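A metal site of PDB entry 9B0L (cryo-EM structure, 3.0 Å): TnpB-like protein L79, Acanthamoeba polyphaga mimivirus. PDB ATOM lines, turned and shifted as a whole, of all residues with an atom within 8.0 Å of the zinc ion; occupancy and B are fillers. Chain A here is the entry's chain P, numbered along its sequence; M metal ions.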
ATOM      1  N   TYR A  57      30.797 -19.452  -9.960  1.00  0.00           N
ATOM      2  CA  TYR A  57      29.669 -18.939 -10.725  1.00  0.00           C
ATOM      3  C   TYR A  57      29.027 -20.052 -11.534  1.00  0.00           C
ATOM      4  O   TYR A  57      29.704 -20.745 -12.300  1.00  0.00           O
ATOM      5  CB  TYR A  57      30.102 -17.807 -11.655  1.00  0.00           C
ATOM      6  CG  TYR A  57      29.190 -17.606 -12.845  1.00  0.00           C
ATOM      7  CD1 TYR A  57      28.063 -16.810 -12.740  1.00  0.00           C
ATOM      8  CD2 TYR A  57      29.461 -18.214 -14.064  1.00  0.00           C
ATOM      9  CE1 TYR A  57      27.226 -16.623 -13.828  1.00  0.00           C
ATOM     10  CE2 TYR A  57      28.634 -18.036 -15.148  1.00  0.00           C
ATOM     11  CZ  TYR A  57      27.518 -17.242 -15.024  1.00  0.00           C
ATOM     12  OH  TYR A  57      26.685 -17.068 -16.101  1.00  0.00           O
ATOM     13  N   LYS A 472      33.335 -11.233  -4.714  1.00  0.00           N
ATOM     14  CA  LYS A 472      33.975 -10.848  -5.972  1.00  0.00           C
ATOM     15  C   LYS A 472      33.177 -11.326  -7.180  1.00  0.00           C
ATOM     16  O   LYS A 472      33.011 -10.580  -8.156  1.00  0.00           O
ATOM     17  CB  LYS A 472      35.395 -11.401  -6.027  1.00  0.00           C
ATOM     18  CG  LYS A 472      36.356 -10.748  -5.068  1.00  0.00           C
ATOM     19  CD  LYS A 472      37.729 -11.387  -5.133  1.00  0.00           C
ATOM     20  CE  LYS A 472      38.722 -10.691  -4.222  1.00  0.00           C
ATOM     21  NZ  LYS A 472      40.048 -11.371  -4.221  1.00  0.00           N
ATOM     22  N   THR A 473      32.676 -12.562  -7.139  1.00  0.00           N
ATOM     23  CA  THR A 473      32.049 -13.141  -8.310  1.00  0.00           C
ATOM     24  C   THR A 473      30.754 -12.419  -8.652  1.00  0.00           C
ATOM     25  O   THR A 473      29.937 -12.116  -7.772  1.00  0.00           O
ATOM     26  CB  THR A 473      31.760 -14.623  -8.070  1.00  0.00           C
ATOM     27  OG1 THR A 473      32.993 -15.313  -7.798  1.00  0.00           O
ATOM     28  CG2 THR A 473      31.117 -15.245  -9.299  1.00  0.00           C
ATOM     29  N   CYS A 474      30.567 -12.144  -9.940  1.00  0.00           N
ATOM     30  CA  CYS A 474      29.325 -11.573 -10.432  1.00  0.00           C
ATOM     31  C   CYS A 474      28.250 -12.634 -10.502  1.00  0.00           C
ATOM     32  O   CYS A 474      28.480 -13.725 -11.050  1.00  0.00           O
ATOM     33  CB  CYS A 474      29.537 -10.938 -11.805  1.00  0.00           C
ATOM     34  SG  CYS A 474      28.016 -10.830 -12.766  1.00  0.00           S
ATOM     35  N   SER A 475      27.068 -12.331  -9.953  1.00  0.00           N
ATOM     36  CA  SER A 475      25.997 -13.305  -9.941  1.00  0.00           C
ATOM     37  C   SER A 475      25.436 -13.561 -11.336  1.00  0.00           C
ATOM     38  O   SER A 475      24.937 -14.652 -11.610  1.00  0.00           O
ATOM     39  CB  SER A 475      24.883 -12.845  -9.006  1.00  0.00           C
ATOM     40  OG  SER A 475      24.369 -11.595  -9.408  1.00  0.00           O
ATOM     41  N   ASN A 476      25.510 -12.575 -12.225  1.00  0.00           N
ATOM     42  CA  ASN A 476      24.895 -12.704 -13.549  1.00  0.00           C
ATOM     43  C   ASN A 476      25.866 -13.266 -14.582  1.00  0.00           C
ATOM     44  O   ASN A 476      25.618 -14.323 -15.171  1.00  0.00           O
ATOM     45  CB  ASN A 476      24.369 -11.345 -14.014  1.00  0.00           C
ATOM     46  CG  ASN A 476      23.394 -10.717 -13.033  1.00  0.00           C
ATOM     47  OD1 ASN A 476      23.175  -9.510 -13.056  1.00  0.00           O
ATOM     48  ND2 ASN A 476      22.800 -11.526 -12.163  1.00  0.00           N
ATOM     49  N   CYS A 477      26.982 -12.564 -14.819  1.00  0.00           N
ATOM     50  CA  CYS A 477      27.893 -12.929 -15.896  1.00  0.00           C
ATOM     51  C   CYS A 477      29.079 -13.763 -15.448  1.00  0.00           C
ATOM     52  O   CYS A 477      29.609 -14.544 -16.243  1.00  0.00           O
ATOM     53  CB  CYS A 477      28.401 -11.664 -16.593  1.00  0.00           C
ATOM     54  SG  CYS A 477      29.952 -11.009 -15.942  1.00  0.00           S
ATOM     55  N   GLY A 478      29.514 -13.611 -14.205  1.00  0.00           N
ATOM     56  CA  GLY A 478      30.611 -14.394 -13.679  1.00  0.00           C
ATOM     57  C   GLY A 478      31.960 -13.701 -13.659  1.00  0.00           C
ATOM     58  O   GLY A 478      32.965 -14.346 -13.360  1.00  0.00           O
ATOM     59  N   LYS A 479      32.009 -12.408 -13.976  1.00  0.00           N
ATOM     60  CA  LYS A 479      33.266 -11.677 -13.873  1.00  0.00           C
ATOM     61  C   LYS A 479      33.676 -11.534 -12.415  1.00  0.00           C
ATOM     62  O   LYS A 479      32.854 -11.219 -11.547  1.00  0.00           O
ATOM     63  CB  LYS A 479      33.115 -10.293 -14.517  1.00  0.00           C
ATOM     64  CG  LYS A 479      33.405 -10.256 -16.018  1.00  0.00           C
ATOM     65  CD  LYS A 479      34.880 -10.533 -16.342  1.00  0.00           C
ATOM     66  CE  LYS A 479      35.826  -9.555 -15.665  1.00  0.00           C
ATOM     67  NZ  LYS A 479      35.308  -8.157 -15.685  1.00  0.00           N
ATOM     68  N   ILE A 480      34.958 -11.769 -12.148  1.00  0.00           N
ATOM     69  CA  ILE A 480      35.495 -11.691 -10.798  1.00  0.00           C
ATOM     70  C   ILE A 480      36.139 -10.316 -10.632  1.00  0.00           C
ATOM     71  O   ILE A 480      37.118  -9.994 -11.303  1.00  0.00           O
ATOM     72  CB  ILE A 480      36.512 -12.807 -10.524  1.00  0.00           C
ATOM     73  CG1 ILE A 480      35.833 -14.179 -10.530  1.00  0.00           C
ATOM     74  CG2 ILE A 480      37.208 -12.580  -9.202  1.00  0.00           C
ATOM     75  CD1 ILE A 480      36.793 -15.358 -10.536  1.00  0.00           C
ATOM     76  N   TYR A 489      27.935  -2.898  -6.018  1.00  0.00           N
ATOM     77  CA  TYR A 489      28.579  -3.812  -6.962  1.00  0.00           C
ATOM     78  C   TYR A 489      28.026  -3.521  -8.351  1.00  0.00           C
ATOM     79  O   TYR A 489      26.837  -3.744  -8.604  1.00  0.00           O
ATOM     80  CB  TYR A 489      28.336  -5.260  -6.555  1.00  0.00           C
ATOM     81  CG  TYR A 489      29.130  -6.264  -7.354  1.00  0.00           C
ATOM     82  CD1 TYR A 489      28.816  -6.543  -8.673  1.00  0.00           C
ATOM     83  CD2 TYR A 489      30.210  -6.933  -6.787  1.00  0.00           C
ATOM     84  CE1 TYR A 489      29.537  -7.457  -9.404  1.00  0.00           C
ATOM     85  CE2 TYR A 489      30.938  -7.847  -7.512  1.00  0.00           C
ATOM     86  CZ  TYR A 489      30.600  -8.115  -8.818  1.00  0.00           C
ATOM     87  OH  TYR A 489      31.329  -9.028  -9.543  1.00  0.00           O
ATOM     88  N   GLU A 490      28.878  -3.012  -9.225  1.00  0.00           N
ATOM     89  CA  GLU A 490      28.493  -2.679 -10.591  1.00  0.00           C
ATOM     90  C   GLU A 490      29.451  -3.405 -11.537  1.00  0.00           C
ATOM     91  O   GLU A 490      30.574  -2.953 -11.754  1.00  0.00           O
ATOM     92  CB  GLU A 490      28.511  -1.167 -10.828  1.00  0.00           C
ATOM     93  CG  GLU A 490      29.772  -0.478 -10.346  1.00  0.00           C
ATOM     94  CD  GLU A 490      29.704   1.024 -10.519  1.00  0.00           C
ATOM     95  OE1 GLU A 490      28.895   1.496 -11.350  1.00  0.00           O
ATOM     96  OE2 GLU A 490      30.450   1.745  -9.816  1.00  0.00           O
ATOM     97  N   CYS A 491      28.994  -4.519 -12.094  1.00  0.00           N
ATOM     98  CA  CYS A 491      29.823  -5.263 -13.036  1.00  0.00           C
ATOM     99  C   CYS A 491      30.058  -4.447 -14.295  1.00  0.00           C
ATOM    100  O   CYS A 491      29.133  -3.834 -14.842  1.00  0.00           O
ATOM    101  CB  CYS A 491      29.159  -6.594 -13.395  1.00  0.00           C
ATOM    102  SG  CYS A 491      30.320  -7.924 -13.761  1.00  0.00           S
ATOM    103  N   GLU A 492      31.305  -4.423 -14.752  1.00  0.00           N
ATOM    104  CA  GLU A 492      31.656  -3.673 -15.958  1.00  0.00           C
ATOM    105  C   GLU A 492      31.318  -4.430 -17.239  1.00  0.00           C
ATOM    106  O   GLU A 492      31.281  -3.817 -18.301  1.00  0.00           O
ATOM    107  CB  GLU A 492      33.146  -3.318 -15.966  1.00  0.00           C
ATOM    108  CG  GLU A 492      33.564  -2.183 -15.032  1.00  0.00           C
ATOM    109  CD  GLU A 492      33.160  -2.420 -13.588  1.00  0.00           C
ATOM    110  OE1 GLU A 492      33.570  -1.613 -12.720  1.00  0.00           O
ATOM    111  OE2 GLU A 492      32.458  -3.408 -13.314  1.00  0.00           O
ATOM    112  N   SER A 493      31.076  -5.733 -17.146  1.00  0.00           N
ATOM    113  CA  SER A 493      30.817  -6.542 -18.342  1.00  0.00           C
ATOM    114  C   SER A 493      29.328  -6.597 -18.669  1.00  0.00           C
ATOM    115  O   SER A 493      28.898  -6.152 -19.725  1.00  0.00           O
ATOM    116  CB  SER A 493      31.385  -7.947 -18.157  1.00  0.00           C
ATOM    117  OG  SER A 493      31.024  -8.794 -19.232  1.00  0.00           O
ATOM    118  N   CYS A 494      28.531  -7.146 -17.746  1.00  0.00           N
ATOM    119  CA  CYS A 494      27.086  -7.249 -17.959  1.00  0.00           C
ATOM    120  C   CYS A 494      26.329  -6.015 -17.515  1.00  0.00           C
ATOM    121  O   CYS A 494      25.149  -5.871 -17.856  1.00  0.00           O
ATOM    122  CB  CYS A 494      26.541  -8.472 -17.218  1.00  0.00           C
ATOM    123  SG  CYS A 494      26.987  -8.509 -15.474  1.00  0.00           S
ATOM    124  N   GLY A 495      26.968  -5.125 -16.759  1.00  0.00           N
ATOM    125  CA  GLY A 495      26.346  -3.884 -16.359  1.00  0.00           C
ATOM    126  C   GLY A 495      25.401  -3.971 -15.185  1.00  0.00           C
ATOM    127  O   GLY A 495      24.726  -2.978 -14.886  1.00  0.00           O
ATOM    128  N   MET A 496      25.310  -5.121 -14.517  1.00  0.00           N
ATOM    129  CA  MET A 496      24.414  -5.230 -13.371  1.00  0.00           C
ATOM    130  C   MET A 496      24.782  -4.186 -12.344  1.00  0.00           C
ATOM    131  O   MET A 496      25.955  -4.001 -12.001  1.00  0.00           O
ATOM    132  CB  MET A 496      24.499  -6.633 -12.770  1.00  0.00           C
ATOM    133  CG  MET A 496      24.382  -6.705 -11.227  1.00  0.00           C
ATOM    134  SD  MET A 496      24.905  -8.278 -10.519  1.00  0.00           S
ATOM    135  CE  MET A 496      26.576  -8.409 -11.148  1.00  0.00           C
ATOM    136  N   ASN A 503      24.295  -9.232  -3.831  1.00  0.00           N
ATOM    137  CA  ASN A 503      24.935 -10.080  -4.827  1.00  0.00           C
ATOM    138  C   ASN A 503      25.659 -11.240  -4.166  1.00  0.00           C
ATOM    139  O   ASN A 503      25.626 -12.376  -4.662  1.00  0.00           O
ATOM    140  CB  ASN A 503      25.911  -9.265  -5.668  1.00  0.00           C
ATOM    141  CG  ASN A 503      26.823 -10.133  -6.489  1.00  0.00           C
ATOM    142  OD1 ASN A 503      26.394 -10.788  -7.433  1.00  0.00           O
ATOM    143  ND2 ASN A 503      28.102 -10.158  -6.127  1.00  0.00           N
HETATM  144 ZN    ZN M   1      28.831  -9.543 -14.508  1.00  0.00          ZN
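The zinc ion is bound by SG of Cys 474, at 2.3 Å. SG of Cys 491 is bound to the zinc ion (2.3 Å). SG of Cys 494 binds the zinc ion (2.3 Å). SG of Cys 477 is bound to the zinc ion (2.3 Å).
N of Gly 478 lies close to SG of Cys 474 (3.5 Å). The backbone NH (N) of Cys 474 is in hydrogen-bond range of the backbone carbonyl oxygen (O) of Lys 479 (2.9 Å). SG of Cys 474 sits close to N of Asn 476, at 3.1 Å. The backbone NH (N) of Cys 474 lies within hydrogen-bond range of the side-chain hydroxyl (OH) of Tyr 489, at 3.2 Å. O of Met 496 lies within hydrogen-bond range of N of Cys 491 (3.1 Å). The side-chain sulfur (SG) of Cys 477 sits close to the backbone NH (N) of Lys 479 (3.2 Å).
Of the 19 residues printed, 4 come within 4 Å of the zinc ion. Along chain A the residues within 4 Å of the zinc ion span positions 474 to 494.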
